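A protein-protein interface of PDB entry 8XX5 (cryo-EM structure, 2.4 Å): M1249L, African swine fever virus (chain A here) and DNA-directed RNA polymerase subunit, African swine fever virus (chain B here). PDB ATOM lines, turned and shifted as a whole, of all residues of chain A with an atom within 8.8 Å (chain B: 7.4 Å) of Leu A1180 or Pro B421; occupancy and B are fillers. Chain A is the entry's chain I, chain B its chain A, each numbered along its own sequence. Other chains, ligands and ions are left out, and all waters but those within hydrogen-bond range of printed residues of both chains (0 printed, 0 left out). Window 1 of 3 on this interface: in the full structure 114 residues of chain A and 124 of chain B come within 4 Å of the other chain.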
ATOM      1  N   PHE A1165      -4.945  18.353  -5.481  1.00  0.00           N
ATOM      2  CA  PHE A1165      -4.784  16.912  -5.602  1.00  0.00           C
ATOM      3  C   PHE A1165      -3.808  16.509  -6.695  1.00  0.00           C
ATOM      4  O   PHE A1165      -3.600  15.310  -6.909  1.00  0.00           O
ATOM      5  CB  PHE A1165      -6.143  16.252  -5.858  1.00  0.00           C
ATOM      6  CG  PHE A1165      -7.043  16.246  -4.663  1.00  0.00           C
ATOM      7  CD1 PHE A1165      -7.818  17.350  -4.358  1.00  0.00           C
ATOM      8  CD2 PHE A1165      -7.112  15.137  -3.839  1.00  0.00           C
ATOM      9  CE1 PHE A1165      -8.645  17.347  -3.256  1.00  0.00           C
ATOM     10  CE2 PHE A1165      -7.938  15.128  -2.738  1.00  0.00           C
ATOM     11  CZ  PHE A1165      -8.704  16.235  -2.445  1.00  0.00           C
ATOM     12  N   SER A1166      -3.206  17.468  -7.392  1.00  0.00           N
ATOM     13  CA  SER A1166      -2.282  17.150  -8.470  1.00  0.00           C
ATOM     14  C   SER A1166      -0.895  16.875  -7.908  1.00  0.00           C
ATOM     15  O   SER A1166      -0.378  17.650  -7.097  1.00  0.00           O
ATOM     16  CB  SER A1166      -2.222  18.295  -9.479  1.00  0.00           C
ATOM     17  OG  SER A1166      -1.686  19.464  -8.887  1.00  0.00           O
ATOM     18  N   ILE A1167      -0.296  15.770  -8.336  1.00  0.00           N
ATOM     19  CA  ILE A1167       1.090  15.454  -7.962  1.00  0.00           C
ATOM     20  C   ILE A1167       1.970  16.110  -9.021  1.00  0.00           C
ATOM     21  O   ILE A1167       2.449  15.488  -9.972  1.00  0.00           O
ATOM     22  CB  ILE A1167       1.323  13.944  -7.825  1.00  0.00           C
ATOM     23  CG1 ILE A1167       0.773  13.193  -9.041  1.00  0.00           C
ATOM     24  CG2 ILE A1167       0.682  13.426  -6.547  1.00  0.00           C
ATOM     25  CD1 ILE A1167       0.758  11.692  -8.878  1.00  0.00           C
ATOM     26  N   ASP A1169       4.443  18.856  -7.900  1.00  0.00           N
ATOM     27  CA  ASP A1169       5.714  19.074  -7.227  1.00  0.00           C
ATOM     28  C   ASP A1169       6.289  17.793  -6.639  1.00  0.00           C
ATOM     29  O   ASP A1169       7.336  17.844  -5.987  1.00  0.00           O
ATOM     30  CB  ASP A1169       5.557  20.128  -6.128  1.00  0.00           C
ATOM     31  CG  ASP A1169       5.515  21.538  -6.679  1.00  0.00           C
ATOM     32  OD1 ASP A1169       5.316  21.692  -7.903  1.00  0.00           O
ATOM     33  OD2 ASP A1169       5.677  22.492  -5.892  1.00  0.00           O
ATOM     34  N   VAL A1170       5.632  16.658  -6.850  1.00  0.00           N
ATOM     35  CA  VAL A1170       6.121  15.363  -6.395  1.00  0.00           C
ATOM     36  C   VAL A1170       6.706  14.647  -7.604  1.00  0.00           C
ATOM     37  O   VAL A1170       5.970  14.197  -8.488  1.00  0.00           O
ATOM     38  CB  VAL A1170       5.010  14.533  -5.742  1.00  0.00           C
ATOM     39  CG1 VAL A1170       5.597  13.314  -5.049  1.00  0.00           C
ATOM     40  CG2 VAL A1170       4.215  15.379  -4.767  1.00  0.00           C
ATOM     41  N   ASP A1171       8.033  14.539  -7.647  1.00  0.00           N
ATOM     42  CA  ASP A1171       8.718  13.855  -8.742  1.00  0.00           C
ATOM     43  C   ASP A1171       8.680  12.355  -8.466  1.00  0.00           C
ATOM     44  O   ASP A1171       9.630  11.751  -7.963  1.00  0.00           O
ATOM     45  CB  ASP A1171      10.144  14.369  -8.894  1.00  0.00           C
ATOM     46  CG  ASP A1171      10.722  14.090 -10.268  1.00  0.00           C
ATOM     47  OD1 ASP A1171      10.329  13.081 -10.890  1.00  0.00           O
ATOM     48  OD2 ASP A1171      11.570  14.881 -10.730  1.00  0.00           O
ATOM     49  N   ILE A1172       7.545  11.749  -8.800  1.00  0.00           N
ATOM     50  CA  ILE A1172       7.331  10.317  -8.644  1.00  0.00           C
ATOM     51  C   ILE A1172       6.936   9.749  -9.999  1.00  0.00           C
ATOM     52  O   ILE A1172       6.097  10.327 -10.699  1.00  0.00           O
ATOM     53  CB  ILE A1172       6.264  10.011  -7.576  1.00  0.00           C
ATOM     54  CG1 ILE A1172       5.953   8.515  -7.533  1.00  0.00           C
ATOM     55  CG2 ILE A1172       5.000  10.826  -7.819  1.00  0.00           C
ATOM     56  CD1 ILE A1172       5.671   7.992  -6.147  1.00  0.00           C
ATOM     57  N   SER A1173       7.562   8.638 -10.378  1.00  0.00           N
ATOM     58  CA  SER A1173       7.251   8.003 -11.650  1.00  0.00           C
ATOM     59  C   SER A1173       5.806   7.525 -11.667  1.00  0.00           C
ATOM     60  O   SER A1173       5.266   7.084 -10.649  1.00  0.00           O
ATOM     61  CB  SER A1173       8.199   6.831 -11.901  1.00  0.00           C
ATOM     62  OG  SER A1173       7.596   5.859 -12.735  1.00  0.00           O
ATOM     63  N   LEU A1174       5.173   7.619 -12.838  1.00  0.00           N
ATOM     64  CA  LEU A1174       3.778   7.218 -12.962  1.00  0.00           C
ATOM     65  C   LEU A1174       3.591   5.715 -12.816  1.00  0.00           C
ATOM     66  O   LEU A1174       2.467   5.264 -12.573  1.00  0.00           O
ATOM     67  CB  LEU A1174       3.208   7.684 -14.303  1.00  0.00           C
ATOM     68  CG  LEU A1174       2.928   9.180 -14.471  1.00  0.00           C
ATOM     69  CD1 LEU A1174       2.389   9.781 -13.181  1.00  0.00           C
ATOM     70  CD2 LEU A1174       4.168   9.928 -14.941  1.00  0.00           C
ATOM     71  N   VAL A1176       5.035   3.867 -10.458  1.00  0.00           N
ATOM     72  CA  VAL A1176       5.137   3.486  -9.055  1.00  0.00           C
ATOM     73  C   VAL A1176       4.123   4.284  -8.250  1.00  0.00           C
ATOM     74  O   VAL A1176       4.345   4.588  -7.073  1.00  0.00           O
ATOM     75  CB  VAL A1176       6.564   3.696  -8.516  1.00  0.00           C
ATOM     76  CG1 VAL A1176       7.524   2.734  -9.183  1.00  0.00           C
ATOM     77  CG2 VAL A1176       7.011   5.131  -8.727  1.00  0.00           C
ATOM     78  N   LEU A1177       3.001   4.626  -8.878  1.00  0.00           N
ATOM     79  CA  LEU A1177       1.964   5.408  -8.220  1.00  0.00           C
ATOM     80  C   LEU A1177       1.259   4.645  -7.108  1.00  0.00           C
ATOM     81  O   LEU A1177       0.557   5.268  -6.304  1.00  0.00           O
ATOM     82  CB  LEU A1177       0.939   5.889  -9.248  1.00  0.00           C
ATOM     83  CG  LEU A1177       1.287   7.208  -9.941  1.00  0.00           C
ATOM     84  CD1 LEU A1177       0.073   7.774 -10.656  1.00  0.00           C
ATOM     85  CD2 LEU A1177       1.843   8.206  -8.941  1.00  0.00           C
ATOM     86  N   ASP A1178       1.423   3.328  -7.035  1.00  0.00           N
ATOM     87  CA  ASP A1178       0.868   2.539  -5.945  1.00  0.00           C
ATOM     88  C   ASP A1178       1.729   2.591  -4.692  1.00  0.00           C
ATOM     89  O   ASP A1178       1.322   2.065  -3.652  1.00  0.00           O
ATOM     90  CB  ASP A1178       0.666   1.090  -6.390  1.00  0.00           C
ATOM     91  CG  ASP A1178      -0.581   0.911  -7.230  1.00  0.00           C
ATOM     92  OD1 ASP A1178      -0.735   1.641  -8.232  1.00  0.00           O
ATOM     93  OD2 ASP A1178      -1.410   0.041  -6.890  1.00  0.00           O
ATOM     94  N   ASN A1179       2.909   3.206  -4.767  1.00  0.00           N
ATOM     95  CA  ASN A1179       3.665   3.526  -3.566  1.00  0.00           C
ATOM     96  C   ASN A1179       2.963   4.566  -2.708  1.00  0.00           C
ATOM     97  O   ASN A1179       3.241   4.652  -1.508  1.00  0.00           O
ATOM     98  CB  ASN A1179       5.063   4.027  -3.934  1.00  0.00           C
ATOM     99  CG  ASN A1179       5.948   2.931  -4.483  1.00  0.00           C
ATOM    100  OD1 ASN A1179       5.468   1.970  -5.077  1.00  0.00           O
ATOM    101  ND2 ASN A1179       7.251   3.074  -4.288  1.00  0.00           N
ATOM    102  N   LEU A1180       2.063   5.352  -3.298  1.00  0.00           N
ATOM    103  CA  LEU A1180       1.256   6.320  -2.576  1.00  0.00           C
ATOM    104  C   LEU A1180      -0.086   5.754  -2.133  1.00  0.00           C
ATOM    105  O   LEU A1180      -0.879   6.487  -1.533  1.00  0.00           O
ATOM    106  CB  LEU A1180       1.022   7.559  -3.447  1.00  0.00           C
ATOM    107  CG  LEU A1180       2.275   8.327  -3.871  1.00  0.00           C
ATOM    108  CD1 LEU A1180       1.920   9.430  -4.851  1.00  0.00           C
ATOM    109  CD2 LEU A1180       2.990   8.892  -2.659  1.00  0.00           C
ATOM    110  N   ALA A1181      -0.354   4.485  -2.415  1.00  0.00           N
ATOM    111  CA  ALA A1181      -1.638   3.896  -2.069  1.00  0.00           C
ATOM    112  C   ALA A1181      -1.803   3.852  -0.552  1.00  0.00           C
ATOM    113  O   ALA A1181      -0.824   3.627   0.172  1.00  0.00           O
ATOM    114  CB  ALA A1181      -1.753   2.486  -2.654  1.00  0.00           C
ATOM    115  N   PRO A1182      -3.011   4.073  -0.036  1.00  0.00           N
ATOM    116  CA  PRO A1182      -3.216   4.024   1.416  1.00  0.00           C
ATOM    117  C   PRO A1182      -2.946   2.630   1.963  1.00  0.00           C
ATOM    118  O   PRO A1182      -3.149   1.624   1.279  1.00  0.00           O
ATOM    119  CB  PRO A1182      -4.686   4.425   1.576  1.00  0.00           C
ATOM    120  CG  PRO A1182      -5.306   4.106   0.254  1.00  0.00           C
ATOM    121  CD  PRO A1182      -4.248   4.424  -0.751  1.00  0.00           C
ATOM    122  N   GLN A1183      -2.479   2.583   3.206  1.00  0.00           N
ATOM    123  CA  GLN A1183      -2.085   1.333   3.847  1.00  0.00           C
ATOM    124  C   GLN A1183      -3.242   0.341   3.914  1.00  0.00           C
ATOM    125  O   GLN A1183      -3.079  -0.844   3.622  1.00  0.00           O
ATOM    126  CB  GLN A1183      -1.555   1.610   5.254  1.00  0.00           C
ATOM    127  CG  GLN A1183      -1.126   0.370   6.011  1.00  0.00           C
ATOM    128  CD  GLN A1183       0.196  -0.176   5.513  1.00  0.00           C
ATOM    129  OE1 GLN A1183       0.320  -1.363   5.219  1.00  0.00           O
ATOM    130  NE2 GLN A1183       1.194   0.693   5.410  1.00  0.00           N
ATOM    131  OXT GLN A1183      -4.369   0.702   4.254  1.00  0.00           O
ATOM    132  N   ASN B 418      16.196   2.625  -3.172  1.00  0.00           N
ATOM    133  CA  ASN B 418      15.429   3.861  -3.141  1.00  0.00           C
ATOM    134  C   ASN B 418      13.953   3.564  -3.347  1.00  0.00           C
ATOM    135  O   ASN B 418      13.589   2.757  -4.204  1.00  0.00           O
ATOM    136  CB  ASN B 418      15.920   4.842  -4.214  1.00  0.00           C
ATOM    137  CG  ASN B 418      14.951   5.979  -4.452  1.00  0.00           C
ATOM    138  OD1 ASN B 418      14.437   6.149  -5.555  1.00  0.00           O
ATOM    139  ND2 ASN B 418      14.694   6.764  -3.415  1.00  0.00           N
ATOM    140  N   ARG B 419      13.108   4.223  -2.559  1.00  0.00           N
ATOM    141  CA  ARG B 419      11.663   4.157  -2.721  1.00  0.00           C
ATOM    142  C   ARG B 419      11.118   5.561  -2.929  1.00  0.00           C
ATOM    143  O   ARG B 419      11.397   6.462  -2.131  1.00  0.00           O
ATOM    144  CB  ARG B 419      10.988   3.511  -1.511  1.00  0.00           C
ATOM    145  CG  ARG B 419       9.548   3.103  -1.768  1.00  0.00           C
ATOM    146  CD  ARG B 419       8.751   3.021  -0.484  1.00  0.00           C
ATOM    147  NE  ARG B 419       8.148   4.300  -0.130  1.00  0.00           N
ATOM    148  CZ  ARG B 419       6.842   4.517  -0.067  1.00  0.00           C
ATOM    149  NH1 ARG B 419       5.969   3.559  -0.329  1.00  0.00           N
ATOM    150  NH2 ARG B 419       6.402   5.725   0.271  1.00  0.00           N
ATOM    151  N   GLN B 420      10.359   5.741  -3.984  1.00  0.00           N
ATOM    152  CA  GLN B 420       9.714   7.027  -4.189  1.00  0.00           C
ATOM    153  C   GLN B 420       8.348   7.049  -3.511  1.00  0.00           C
ATOM    154  O   GLN B 420       7.664   6.023  -3.446  1.00  0.00           O
ATOM    155  CB  GLN B 420       9.552   7.308  -5.678  1.00  0.00           C
ATOM    156  CG  GLN B 420      10.849   7.244  -6.458  1.00  0.00           C
ATOM    157  CD  GLN B 420      10.643   7.463  -7.940  1.00  0.00           C
ATOM    158  OE1 GLN B 420      10.490   6.511  -8.705  1.00  0.00           O
ATOM    159  NE2 GLN B 420      10.639   8.724  -8.354  1.00  0.00           N
ATOM    160  N   PRO B 421       7.913   8.205  -2.995  1.00  0.00           N
ATOM    161  CA  PRO B 421       8.588   9.511  -3.000  1.00  0.00           C
ATOM    162  C   PRO B 421       9.759   9.579  -2.023  1.00  0.00           C
ATOM    163  O   PRO B 421       9.659   9.140  -0.883  1.00  0.00           O
ATOM    164  CB  PRO B 421       7.460  10.476  -2.611  1.00  0.00           C
ATOM    165  CG  PRO B 421       6.552   9.658  -1.755  1.00  0.00           C
ATOM    166  CD  PRO B 421       6.593   8.274  -2.344  1.00  0.00           C
ATOM    167  N   SER B 422      10.884  10.137  -2.461  1.00  0.00           N
ATOM    168  CA  SER B 422      12.088  10.220  -1.638  1.00  0.00           C
ATOM    169  C   SER B 422      12.003  11.476  -0.785  1.00  0.00           C
ATOM    170  O   SER B 422      12.363  12.569  -1.227  1.00  0.00           O
ATOM    171  CB  SER B 422      13.335  10.225  -2.514  1.00  0.00           C
ATOM    172  OG  SER B 422      13.216   9.293  -3.572  1.00  0.00           O
ATOM    173  N   LEU B 423      11.528  11.322   0.452  1.00  0.00           N
ATOM    174  CA  LEU B 423      11.268  12.458   1.322  1.00  0.00           C
ATOM    175  C   LEU B 423      12.237  12.580   2.488  1.00  0.00           C
ATOM    176  O   LEU B 423      12.362  13.672   3.048  1.00  0.00           O
ATOM    177  CB  LEU B 423       9.838  12.382   1.874  1.00  0.00           C
ATOM    178  CG  LEU B 423       8.727  12.565   0.841  1.00  0.00           C
ATOM    179  CD1 LEU B 423       7.442  11.911   1.316  1.00  0.00           C
ATOM    180  CD2 LEU B 423       8.508  14.037   0.547  1.00  0.00           C
ATOM    181  N   GLU B 424      12.916  11.504   2.865  1.00  0.00           N
ATOM    182  CA  GLU B 424      13.824  11.502   4.001  1.00  0.00           C
ATOM    183  C   GLU B 424      15.263  11.336   3.536  1.00  0.00           C
ATOM    184  O   GLU B 424      15.540  10.957   2.396  1.00  0.00           O
ATOM    185  CB  GLU B 424      13.461  10.385   4.987  1.00  0.00           C
ATOM    186  CG  GLU B 424      12.083  10.508   5.601  1.00  0.00           C
ATOM    187  CD  GLU B 424      12.087  11.341   6.869  1.00  0.00           C
ATOM    188  OE1 GLU B 424      12.546  12.504   6.824  1.00  0.00           O
ATOM    189  OE2 GLU B 424      11.633  10.832   7.915  1.00  0.00           O
ATOM    190  N   SER B 427      15.742   7.850   2.504  1.00  0.00           N
ATOM    191  CA  SER B 427      14.974   7.354   1.369  1.00  0.00           C
ATOM    192  C   SER B 427      15.854   6.655   0.346  1.00  0.00           C
ATOM    193  O   SER B 427      15.356   5.825  -0.420  1.00  0.00           O
ATOM    194  CB  SER B 427      14.211   8.498   0.707  1.00  0.00           C
ATOM    195  OG  SER B 427      13.113   8.904   1.501  1.00  0.00           O
ATOM    196  N   TYR B 454      12.564   3.685   4.507  1.00  0.00           N
ATOM    197  CA  TYR B 454      11.922   4.102   3.272  1.00  0.00           C
ATOM    198  C   TYR B 454      10.432   4.363   3.418  1.00  0.00           C
ATOM    199  O   TYR B 454       9.791   4.743   2.433  1.00  0.00           O
ATOM    200  CB  TYR B 454      12.150   3.046   2.188  1.00  0.00           C
ATOM    201  CG  TYR B 454      13.585   2.597   2.083  1.00  0.00           C
ATOM    202  CD1 TYR B 454      14.528   3.377   1.433  1.00  0.00           C
ATOM    203  CD2 TYR B 454      13.997   1.395   2.637  1.00  0.00           C
ATOM    204  CE1 TYR B 454      15.839   2.971   1.334  1.00  0.00           C
ATOM    205  CE2 TYR B 454      15.308   0.981   2.544  1.00  0.00           C
ATOM    206  CZ  TYR B 454      16.225   1.774   1.892  1.00  0.00           C
ATOM    207  OH  TYR B 454      17.531   1.370   1.794  1.00  0.00           O
ATOM    208  N   ASN B 455       9.869   4.182   4.613  1.00  0.00           N
ATOM    209  CA  ASN B 455       8.422   4.262   4.820  1.00  0.00           C
ATOM    210  C   ASN B 455       7.698   3.309   3.873  1.00  0.00           C
ATOM    211  O   ASN B 455       6.690   3.653   3.252  1.00  0.00           O
ATOM    212  CB  ASN B 455       7.920   5.698   4.657  1.00  0.00           C
ATOM    213  CG  ASN B 455       6.529   5.896   5.221  1.00  0.00           C
ATOM    214  OD1 ASN B 455       6.169   5.309   6.240  1.00  0.00           O
ATOM    215  ND2 ASN B 455       5.735   6.728   4.555  1.00  0.00           N
ATOM    216  N   ASP B 461       4.387  -1.980  -3.157  1.00  0.00           N
ATOM    217  CA  ASP B 461       5.410  -0.951  -3.286  1.00  0.00           C
ATOM    218  C   ASP B 461       6.533  -1.417  -4.200  1.00  0.00           C
ATOM    219  O   ASP B 461       6.941  -2.580  -4.164  1.00  0.00           O
ATOM    220  CB  ASP B 461       5.968  -0.592  -1.908  1.00  0.00           C
ATOM    221  CG  ASP B 461       5.031   0.288  -1.112  1.00  0.00           C
ATOM    222  OD1 ASP B 461       3.804   0.080  -1.194  1.00  0.00           O
ATOM    223  OD2 ASP B 461       5.519   1.191  -0.403  1.00  0.00           O
ATOM    224  N   GLN B 462       7.023  -0.502  -5.028  1.00  0.00           N
ATOM    225  CA  GLN B 462       8.142  -0.759  -5.919  1.00  0.00           C
ATOM    226  C   GLN B 462       9.313   0.129  -5.531  1.00  0.00           C
ATOM    227  O   GLN B 462       9.131   1.307  -5.209  1.00  0.00           O
ATOM    228  CB  GLN B 462       7.760  -0.507  -7.377  1.00  0.00           C
ATOM    229  CG  GLN B 462       6.633  -1.375  -7.879  1.00  0.00           C
ATOM    230  CD  GLN B 462       6.460  -1.276  -9.377  1.00  0.00           C
ATOM    231  OE1 GLN B 462       7.304  -1.741 -10.142  1.00  0.00           O
ATOM    232  NE2 GLN B 462       5.364  -0.667  -9.805  1.00  0.00           N
ATOM    233  N   LYS B 815      -5.634  11.613   2.948  1.00  0.00           N
ATOM    234  CA  LYS B 815      -4.448  10.862   2.552  1.00  0.00           C
ATOM    235  C   LYS B 815      -4.039  11.194   1.121  1.00  0.00           C
ATOM    236  O   LYS B 815      -2.847  11.337   0.826  1.00  0.00           O
ATOM    237  CB  LYS B 815      -4.702   9.363   2.708  1.00  0.00           C
ATOM    238  CG  LYS B 815      -3.761   8.478   1.908  1.00  0.00           C
ATOM    239  CD  LYS B 815      -2.344   8.530   2.455  1.00  0.00           C
ATOM    240  CE  LYS B 815      -1.606   7.229   2.194  1.00  0.00           C
ATOM    241  NZ  LYS B 815      -0.409   7.428   1.333  1.00  0.00           N
ATOM    242  N   ALA B 816      -5.014  11.321   0.221  1.00  0.00           N
ATOM    243  CA  ALA B 816      -4.702  11.604  -1.175  1.00  0.00           C
ATOM    244  C   ALA B 816      -4.077  12.983  -1.336  1.00  0.00           C
ATOM    245  O   ALA B 816      -3.047  13.132  -2.003  1.00  0.00           O
ATOM    246  CB  ALA B 816      -5.964  11.485  -2.028  1.00  0.00           C
ATOM    247  N   THR B 819      -0.259  13.953  -0.012  1.00  0.00           N
ATOM    248  CA  THR B 819       0.889  13.798  -0.898  1.00  0.00           C
ATOM    249  C   THR B 819       1.131  15.064  -1.707  1.00  0.00           C
ATOM    250  O   THR B 819       2.260  15.558  -1.783  1.00  0.00           O
ATOM    251  CB  THR B 819       0.681  12.602  -1.827  1.00  0.00           C
ATOM    252  OG1 THR B 819       0.458  11.421  -1.049  1.00  0.00           O
ATOM    253  CG2 THR B 819       1.900  12.402  -2.711  1.00  0.00           C
ATOM    254  N   SER B 820       0.073  15.626  -2.293  1.00  0.00           N
ATOM    255  CA  SER B 820       0.234  16.804  -3.139  1.00  0.00           C
ATOM    256  C   SER B 820       0.635  18.028  -2.323  1.00  0.00           C
ATOM    257  O   SER B 820       1.538  18.777  -2.716  1.00  0.00           O
ATOM    258  CB  SER B 820      -1.054  17.069  -3.915  1.00  0.00           C
ATOM    259  OG  SER B 820      -2.191  16.713  -3.153  1.00  0.00           O
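Among the printed residues, pairs that only touch across the chains: Phe A1165 with Ser B820, Ser A1166 with Ser B820, Val A1170 with Thr B819, Ile A1172 with Gln B420, Ile A1172 with Pro B421, Ser A1173 with Gln B420, Val A1176 with Gln B420, Val A1176 with Gln B462, Asn A1179 with Asp B461, Leu A1180 with Pro B421, Leu A1180 with Thr B819, Ala A1181 with Lys B815 and Pro A1182 with Lys B815.
O of Ser B427 sits at hydrogen-bond distance from N of Arg B419, at 3.5 Å.
NH1 of Arg B419 lies within salt-bridge range of OD2 of Asp B461 (2.4 Å).
The guanidinium group of Arg B419 lies within hydrogen-bond range of the backbone carbonyl oxygen of Tyr B454, at 3.1 Å.
The side-chain amide oxygen (OD1) of Asn A1179 sits close to the backbone carbonyl oxygen (O) of Val A1176.
Of the 17 printed residues of chain A, 11 touch a printed residue of chain B.
Printed residues of chain A that touch a printed residue of chain B: Phe A1165, Ser A1166, Val A1170, Asp A1171, Ile A1172, Ser A1173, Val A1176, Asn A1179, Leu A1180, Ala A1181 and Pro A1182.
Hydrophobic or aromatic side chains of chain A within 4 Å of the printed part of chain B: Val A1170, Ile A1172, Val A1176 and Leu A1180.
Along chain A the printed residues that touch a printed residue of chain B span positions 1165 to 1182.
Leu A1180 touches just these residues of chain B: Pro B421, Lys B815 and Thr B819.
Printed residues of chain B within 4 Å of Ala A1181: Lys B815 (3.996 Å).
Printed residues of chain A within 4 Å of Pro B421: Ile A1172 (3.9 Å) and Leu A1180 (3.7 Å).
Printed residues of chain A within 4 Å of Thr B819: Val A1170 and Leu A1180.
The nearest residue of chain B that does not touch Leu A1180 is Arg B419 (5.2 Å).
The nearest printed residue of chain B that does not touch Ile A1172 is Thr B819 (6.2 Å).
The backbone carbonyl oxygen (O) of Leu A1180 sits at hydrogen-bond distance from the side-chain amino group (NZ) of Lys B815 (3.1 Å).
The backbone carbonyl oxygen (O) of Asn A1179 lies within hydrogen-bond range of the guanidinium group (NH1) of Arg B419 (3.2 Å).
The side-chain amide nitrogen of Asn A1179 lies within hydrogen-bond range of the backbone carbonyl oxygen of Gln B462 (2.7 Å).
NE2 of Gln B420 sits at hydrogen-bond distance from O of Asp A1171 (3.2 Å).
ND2 of Asn A1179 sits at hydrogen-bond distance from O of Gln B420 (3.1 Å).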
